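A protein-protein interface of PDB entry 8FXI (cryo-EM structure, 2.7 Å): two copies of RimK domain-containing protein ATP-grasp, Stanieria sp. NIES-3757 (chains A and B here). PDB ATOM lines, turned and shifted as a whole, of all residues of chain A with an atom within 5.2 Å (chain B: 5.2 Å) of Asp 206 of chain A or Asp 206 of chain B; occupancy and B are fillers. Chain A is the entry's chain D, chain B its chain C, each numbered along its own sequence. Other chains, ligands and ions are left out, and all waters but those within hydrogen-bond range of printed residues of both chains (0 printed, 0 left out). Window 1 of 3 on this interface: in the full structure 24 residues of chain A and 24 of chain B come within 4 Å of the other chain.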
ATOM      1  N   THR A 201       9.256   5.062   1.533  1.00  0.00           N
ATOM      2  CA  THR A 201       9.827   4.413   2.704  1.00  0.00           C
ATOM      3  C   THR A 201      11.206   3.813   2.453  1.00  0.00           C
ATOM      4  O   THR A 201      11.724   3.103   3.318  1.00  0.00           O
ATOM      5  CB  THR A 201       8.876   3.334   3.231  1.00  0.00           C
ATOM      6  OG1 THR A 201       8.637   2.363   2.209  1.00  0.00           O
ATOM      7  CG2 THR A 201       7.571   3.942   3.664  1.00  0.00           C
ATOM      8  N   THR A 202      11.790   4.054   1.283  1.00  0.00           N
ATOM      9  CA  THR A 202      13.182   3.709   1.035  1.00  0.00           C
ATOM     10  C   THR A 202      14.085   4.891   1.360  1.00  0.00           C
ATOM     11  O   THR A 202      13.766   6.034   1.034  1.00  0.00           O
ATOM     12  CB  THR A 202      13.373   3.301  -0.423  1.00  0.00           C
ATOM     13  OG1 THR A 202      12.288   2.461  -0.826  1.00  0.00           O
ATOM     14  CG2 THR A 202      14.672   2.551  -0.605  1.00  0.00           C
ATOM     15  N   PHE A 203      15.223   4.618   1.988  1.00  0.00           N
ATOM     16  CA  PHE A 203      16.166   5.659   2.374  1.00  0.00           C
ATOM     17  C   PHE A 203      17.555   5.338   1.840  1.00  0.00           C
ATOM     18  O   PHE A 203      17.813   4.249   1.327  1.00  0.00           O
ATOM     19  CB  PHE A 203      16.196   5.836   3.896  1.00  0.00           C
ATOM     20  CG  PHE A 203      14.894   6.301   4.469  1.00  0.00           C
ATOM     21  CD1 PHE A 203      14.573   7.642   4.486  1.00  0.00           C
ATOM     22  CD2 PHE A 203      13.986   5.399   4.980  1.00  0.00           C
ATOM     23  CE1 PHE A 203      13.376   8.071   5.003  1.00  0.00           C
ATOM     24  CE2 PHE A 203      12.789   5.826   5.501  1.00  0.00           C
ATOM     25  CZ  PHE A 203      12.485   7.162   5.511  1.00  0.00           C
ATOM     26  N   ASP A 204      18.461   6.304   1.967  1.00  0.00           N
ATOM     27  CA  ASP A 204      19.772   6.199   1.339  1.00  0.00           C
ATOM     28  C   ASP A 204      20.768   5.389   2.154  1.00  0.00           C
ATOM     29  O   ASP A 204      21.907   5.222   1.712  1.00  0.00           O
ATOM     30  CB  ASP A 204      20.348   7.593   1.064  1.00  0.00           C
ATOM     31  CG  ASP A 204      20.616   8.374   2.331  1.00  0.00           C
ATOM     32  OD1 ASP A 204      20.012   8.045   3.368  1.00  0.00           O
ATOM     33  OD2 ASP A 204      21.422   9.327   2.295  1.00  0.00           O
ATOM     34  N   VAL A 205      20.385   4.888   3.330  1.00  0.00           N
ATOM     35  CA  VAL A 205      21.267   4.048   4.127  1.00  0.00           C
ATOM     36  C   VAL A 205      21.029   2.563   3.890  1.00  0.00           C
ATOM     37  O   VAL A 205      21.752   1.734   4.452  1.00  0.00           O
ATOM     38  CB  VAL A 205      21.131   4.376   5.624  1.00  0.00           C
ATOM     39  CG1 VAL A 205      21.646   5.763   5.898  1.00  0.00           C
ATOM     40  CG2 VAL A 205      19.689   4.264   6.051  1.00  0.00           C
ATOM     41  N   ASP A 206      20.039   2.205   3.081  1.00  0.00           N
ATOM     42  CA  ASP A 206      19.753   0.812   2.788  1.00  0.00           C
ATOM     43  C   ASP A 206      20.743   0.260   1.769  1.00  0.00           C
ATOM     44  O   ASP A 206      21.356   0.998   1.001  1.00  0.00           O
ATOM     45  CB  ASP A 206      18.323   0.665   2.280  1.00  0.00           C
ATOM     46  CG  ASP A 206      17.310   1.205   3.257  1.00  0.00           C
ATOM     47  OD1 ASP A 206      17.729   1.719   4.311  1.00  0.00           O
ATOM     48  OD2 ASP A 206      16.099   1.114   2.983  1.00  0.00           O
ATOM     49  N   SER A 207      20.883  -1.062   1.762  1.00  0.00           N
ATOM     50  CA  SER A 207      21.900  -1.728   0.963  1.00  0.00           C
ATOM     51  C   SER A 207      21.370  -2.158  -0.396  1.00  0.00           C
ATOM     52  O   SER A 207      20.199  -2.501  -0.554  1.00  0.00           O
ATOM     53  CB  SER A 207      22.446  -2.951   1.690  1.00  0.00           C
ATOM     54  OG  SER A 207      23.311  -2.563   2.734  1.00  0.00           O
ATOM     55  N   HIS A 208      22.268  -2.150  -1.377  1.00  0.00           N
ATOM     56  CA  HIS A 208      21.952  -2.616  -2.720  1.00  0.00           C
ATOM     57  C   HIS A 208      21.877  -4.133  -2.788  1.00  0.00           C
ATOM     58  O   HIS A 208      21.175  -4.677  -3.644  1.00  0.00           O
ATOM     59  CB  HIS A 208      23.003  -2.090  -3.697  1.00  0.00           C
ATOM     60  CG  HIS A 208      22.766  -2.479  -5.121  1.00  0.00           C
ATOM     61  ND1 HIS A 208      21.608  -2.164  -5.797  1.00  0.00           N
ATOM     62  CD2 HIS A 208      23.547  -3.145  -6.002  1.00  0.00           C
ATOM     63  CE1 HIS A 208      21.684  -2.624  -7.032  1.00  0.00           C
ATOM     64  NE2 HIS A 208      22.849  -3.225  -7.180  1.00  0.00           N
ATOM     65  N   ARG A 423      20.475  -5.174   6.421  1.00  0.00           N
ATOM     66  CA  ARG A 423      20.752  -3.744   6.554  1.00  0.00           C
ATOM     67  C   ARG A 423      19.660  -2.934   5.857  1.00  0.00           C
ATOM     68  O   ARG A 423      19.882  -2.248   4.864  1.00  0.00           O
ATOM     69  CB  ARG A 423      22.132  -3.415   5.999  1.00  0.00           C
ATOM     70  CG  ARG A 423      23.270  -3.980   6.809  1.00  0.00           C
ATOM     71  CD  ARG A 423      24.604  -3.653   6.178  1.00  0.00           C
ATOM     72  NE  ARG A 423      24.925  -2.234   6.253  1.00  0.00           N
ATOM     73  CZ  ARG A 423      25.729  -1.699   7.158  1.00  0.00           C
ATOM     74  NH1 ARG A 423      26.311  -2.436   8.089  1.00  0.00           N
ATOM     75  NH2 ARG A 423      25.959  -0.390   7.129  1.00  0.00           N
ATOM     76  N   LEU A 424      18.456  -3.031   6.409  1.00  0.00           N
ATOM     77  CA  LEU A 424      17.302  -2.288   5.935  1.00  0.00           C
ATOM     78  C   LEU A 424      16.632  -1.619   7.123  1.00  0.00           C
ATOM     79  O   LEU A 424      16.703  -2.111   8.248  1.00  0.00           O
ATOM     80  CB  LEU A 424      16.305  -3.192   5.219  1.00  0.00           C
ATOM     81  CG  LEU A 424      16.857  -4.072   4.102  1.00  0.00           C
ATOM     82  CD1 LEU A 424      15.802  -5.040   3.634  1.00  0.00           C
ATOM     83  CD2 LEU A 424      17.336  -3.226   2.955  1.00  0.00           C
ATOM     84  N   THR A 425      15.984  -0.485   6.870  1.00  0.00           N
ATOM     85  CA  THR A 425      15.367   0.251   7.964  1.00  0.00           C
ATOM     86  C   THR A 425      14.001  -0.316   8.328  1.00  0.00           C
ATOM     87  O   THR A 425      13.693  -0.475   9.512  1.00  0.00           O
ATOM     88  CB  THR A 425      15.245   1.729   7.601  1.00  0.00           C
ATOM     89  OG1 THR A 425      16.522   2.218   7.180  1.00  0.00           O
ATOM     90  CG2 THR A 425      14.783   2.529   8.798  1.00  0.00           C
ATOM     91  N   THR B 201      33.800  -6.018  -6.538  1.00  0.00           N
ATOM     92  CA  THR B 201      34.093  -4.694  -6.009  1.00  0.00           C
ATOM     93  C   THR B 201      32.866  -3.976  -5.460  1.00  0.00           C
ATOM     94  O   THR B 201      32.955  -2.790  -5.130  1.00  0.00           O
ATOM     95  CB  THR B 201      34.768  -3.832  -7.081  1.00  0.00           C
ATOM     96  OG1 THR B 201      33.909  -3.719  -8.218  1.00  0.00           O
ATOM     97  CG2 THR B 201      36.081  -4.434  -7.497  1.00  0.00           C
ATOM     98  N   THR B 202      31.724  -4.653  -5.388  1.00  0.00           N
ATOM     99  CA  THR B 202      30.562  -4.126  -4.685  1.00  0.00           C
ATOM    100  C   THR B 202      30.559  -4.605  -3.240  1.00  0.00           C
ATOM    101  O   THR B 202      30.853  -5.767  -2.961  1.00  0.00           O
ATOM    102  CB  THR B 202      29.279  -4.573  -5.378  1.00  0.00           C
ATOM    103  OG1 THR B 202      29.439  -4.455  -6.794  1.00  0.00           O
ATOM    104  CG2 THR B 202      28.108  -3.721  -4.942  1.00  0.00           C
ATOM    105  N   PHE B 203      30.209  -3.715  -2.317  1.00  0.00           N
ATOM    106  CA  PHE B 203      30.184  -4.039  -0.897  1.00  0.00           C
ATOM    107  C   PHE B 203      28.826  -3.693  -0.301  1.00  0.00           C
ATOM    108  O   PHE B 203      27.985  -3.061  -0.938  1.00  0.00           O
ATOM    109  CB  PHE B 203      31.307  -3.314  -0.149  1.00  0.00           C
ATOM    110  CG  PHE B 203      32.679  -3.726  -0.586  1.00  0.00           C
ATOM    111  CD1 PHE B 203      33.277  -4.850  -0.056  1.00  0.00           C
ATOM    112  CD2 PHE B 203      33.365  -2.997  -1.532  1.00  0.00           C
ATOM    113  CE1 PHE B 203      34.531  -5.234  -0.461  1.00  0.00           C
ATOM    114  CE2 PHE B 203      34.621  -3.379  -1.938  1.00  0.00           C
ATOM    115  CZ  PHE B 203      35.203  -4.498  -1.402  1.00  0.00           C
ATOM    116  N   ASP B 204      28.617  -4.115   0.944  1.00  0.00           N
ATOM    117  CA  ASP B 204      27.304  -4.010   1.567  1.00  0.00           C
ATOM    118  C   ASP B 204      27.026  -2.639   2.163  1.00  0.00           C
ATOM    119  O   ASP B 204      25.937  -2.433   2.705  1.00  0.00           O
ATOM    120  CB  ASP B 204      27.138  -5.083   2.649  1.00  0.00           C
ATOM    121  CG  ASP B 204      28.100  -4.903   3.802  1.00  0.00           C
ATOM    122  OD1 ASP B 204      29.134  -4.237   3.612  1.00  0.00           O
ATOM    123  OD2 ASP B 204      27.833  -5.434   4.900  1.00  0.00           O
ATOM    124  N   VAL B 205      27.969  -1.701   2.092  1.00  0.00           N
ATOM    125  CA  VAL B 205      27.742  -0.348   2.582  1.00  0.00           C
ATOM    126  C   VAL B 205      27.301   0.605   1.480  1.00  0.00           C
ATOM    127  O   VAL B 205      27.008   1.771   1.765  1.00  0.00           O
ATOM    128  CB  VAL B 205      28.997   0.198   3.286  1.00  0.00           C
ATOM    129  CG1 VAL B 205      29.261  -0.579   4.547  1.00  0.00           C
ATOM    130  CG2 VAL B 205      30.187   0.114   2.365  1.00  0.00           C
ATOM    131  N   ASP B 206      27.247   0.147   0.235  1.00  0.00           N
ATOM    132  CA  ASP B 206      26.821   0.983  -0.873  1.00  0.00           C
ATOM    133  C   ASP B 206      25.303   1.123  -0.893  1.00  0.00           C
ATOM    134  O   ASP B 206      24.572   0.294  -0.354  1.00  0.00           O
ATOM    135  CB  ASP B 206      27.323   0.405  -2.190  1.00  0.00           C
ATOM    136  CG  ASP B 206      28.822   0.244  -2.212  1.00  0.00           C
ATOM    137  OD1 ASP B 206      29.458   0.555  -1.188  1.00  0.00           O
ATOM    138  OD2 ASP B 206      29.369  -0.185  -3.245  1.00  0.00           O
ATOM    139  N   SER B 207      24.833   2.186  -1.537  1.00  0.00           N
ATOM    140  CA  SER B 207      23.423   2.546  -1.510  1.00  0.00           C
ATOM    141  C   SER B 207      22.662   1.966  -2.692  1.00  0.00           C
ATOM    142  O   SER B 207      23.195   1.810  -3.790  1.00  0.00           O
ATOM    143  CB  SER B 207      23.250   4.060  -1.504  1.00  0.00           C
ATOM    144  OG  SER B 207      23.560   4.591  -0.236  1.00  0.00           O
ATOM    145  N   HIS B 208      21.389   1.666  -2.447  1.00  0.00           N
ATOM    146  CA  HIS B 208      20.494   1.185  -3.490  1.00  0.00           C
ATOM    147  C   HIS B 208      20.060   2.303  -4.423  1.00  0.00           C
ATOM    148  O   HIS B 208      19.737   2.046  -5.586  1.00  0.00           O
ATOM    149  CB  HIS B 208      19.275   0.527  -2.843  1.00  0.00           C
ATOM    150  CG  HIS B 208      18.293  -0.036  -3.819  1.00  0.00           C
ATOM    151  ND1 HIS B 208      18.632  -0.990  -4.751  1.00  0.00           N
ATOM    152  CD2 HIS B 208      16.975   0.210  -3.996  1.00  0.00           C
ATOM    153  CE1 HIS B 208      17.567  -1.304  -5.465  1.00  0.00           C
ATOM    154  NE2 HIS B 208      16.549  -0.588  -5.027  1.00  0.00           N
ATOM    155  N   ARG B 423      27.264   7.879  -2.215  1.00  0.00           N
ATOM    156  CA  ARG B 423      27.592   6.921  -1.160  1.00  0.00           C
ATOM    157  C   ARG B 423      28.016   5.589  -1.777  1.00  0.00           C
ATOM    158  O   ARG B 423      27.358   4.562  -1.642  1.00  0.00           O
ATOM    159  CB  ARG B 423      26.411   6.748  -0.214  1.00  0.00           C
ATOM    160  CG  ARG B 423      26.108   7.966   0.621  1.00  0.00           C
ATOM    161  CD  ARG B 423      24.900   7.739   1.501  1.00  0.00           C
ATOM    162  NE  ARG B 423      25.154   6.770   2.557  1.00  0.00           N
ATOM    163  CZ  ARG B 423      25.446   7.092   3.809  1.00  0.00           C
ATOM    164  NH1 ARG B 423      25.534   8.352   4.197  1.00  0.00           N
ATOM    165  NH2 ARG B 423      25.652   6.124   4.697  1.00  0.00           N
ATOM    166  N   LEU B 424      29.149   5.631  -2.467  1.00  0.00           N
ATOM    167  CA  LEU B 424      29.754   4.459  -3.073  1.00  0.00           C
ATOM    168  C   LEU B 424      31.223   4.414  -2.689  1.00  0.00           C
ATOM    169  O   LEU B 424      31.846   5.448  -2.450  1.00  0.00           O
ATOM    170  CB  LEU B 424      29.616   4.475  -4.592  1.00  0.00           C
ATOM    171  CG  LEU B 424      28.213   4.690  -5.150  1.00  0.00           C
ATOM    172  CD1 LEU B 424      28.270   4.878  -6.643  1.00  0.00           C
ATOM    173  CD2 LEU B 424      27.326   3.525  -4.804  1.00  0.00           C
ATOM    174  N   THR B 425      31.775   3.206  -2.622  1.00  0.00           N
ATOM    175  CA  THR B 425      33.164   3.071  -2.200  1.00  0.00           C
ATOM    176  C   THR B 425      34.130   3.327  -3.349  1.00  0.00           C
ATOM    177  O   THR B 425      35.130   4.027  -3.171  1.00  0.00           O
ATOM    178  CB  THR B 425      33.401   1.685  -1.608  1.00  0.00           C
ATOM    179  OG1 THR B 425      32.427   1.433  -0.591  1.00  0.00           O
ATOM    180  CG2 THR B 425      34.782   1.603  -0.997  1.00  0.00           C
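Arg 423 of chain B touches Asp 204 of chain A.
O of Asp 206 of chain A touches O of Asp 206 of chain B, 3.6 Å away.
Ser 207 of chain B touches Asp 206 of chain A (CA to O, 3.6 Å).
Asp 206 of chain A touches His 208 of chain B (O to N, 3.5 Å).
Ser 207 of chain A touches Asp 206 of chain B.
Ser 207 of chain A touches His 208 of chain B (O to CB, 3.9 Å).
N of His 208 of chain A touches O of Asp 206 of chain B, at 3.5 Å.
His 208 of chain A touches Ser 207 of chain B (CB to O, 3.9 Å).
Asp 204 of chain B touches Arg 423 of chain A.
The side-chain hydroxyl (OG) of Ser 207 of chain B is in hydrogen-bond range of the backbone carbonyl oxygen (O) of Asp 204 of chain A (2.6 Å).
A ring nitrogen (ND1) of His 208 of chain B sits at hydrogen-bond distance from a ring nitrogen (ND1) of His 208 of chain A (3.4 Å).
OG of Ser 207 of chain A sits at hydrogen-bond distance from O of Asp 204 of chain B (2.6 Å).
Asp 204 of chain A touches Ser 207 of chain B, and with the chains exchanged Ser 207 of chain A touches Asp 204 of chain B.
Asp 204 of chain A touches Arg 423 of chain B, and with the chains exchanged Arg 423 of chain A touches Asp 204 of chain B.
Asp 206 of chain A touches its own counterpart, Asp 206 of chain B.
Asp 206 of chain A touches Ser 207 of chain B, and with the chains exchanged Ser 207 of chain A touches Asp 206 of chain B.
Positions printed for both chains: 201, 202, 203, 204, 205, 206, 207, 208, 423, 424 and 425.
Of the 11 printed residues of chain B, 5 touch a printed residue of chain A.
Asp 206 of chain A touches just these residues of chain B: Asp 206, Ser 207 and His 208.
Asp 206 of chain B touches three residues of chain A.
Of the printed residues of chain B, Asp 204 of chain A touches Ser 207 and Arg 423.
Printed residues of chain A within 4 Å of Asp 204 of chain B: Ser 207 and Arg 423.
Printed residues of chain B within 4 Å of His 208 of chain A: Asp 206 (3.5 Å), Ser 207 (3.9 Å) and His 208 (3.4 Å).
Of the printed residues of chain B, Arg 423 of chain A touches Asp 204 (3.7 Å).
Printed residues of chain A within 4 Å of His 208 of chain B: Asp 206, Ser 207 and His 208.
The nearest printed residue of chain B that does not touch Asp 206 of chain A is Val 205 of chain B (5.8 Å).
The nearest printed residue of chain B that does not touch Arg 423 of chain A is Val 205 of chain B (4.2 Å).
OG1 of Thr 425 of chain A sits at hydrogen-bond distance from OD1 of Asp 206 of chain A (3.2 Å).
The backbone carbonyl oxygen (O) of Arg 423 of chain A lies within hydrogen-bond range of the backbone NH (N) of Ser 207 of chain A (3.5 Å).
O of Arg 423 of chain B sits at hydrogen-bond distance from N of Ser 207 of chain B.
The side-chain hydroxyl (OG1) of Thr 425 of chain B is in hydrogen-bond range of the side-chain carboxylate (OD1) of Asp 206 of chain B (3.2 Å).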
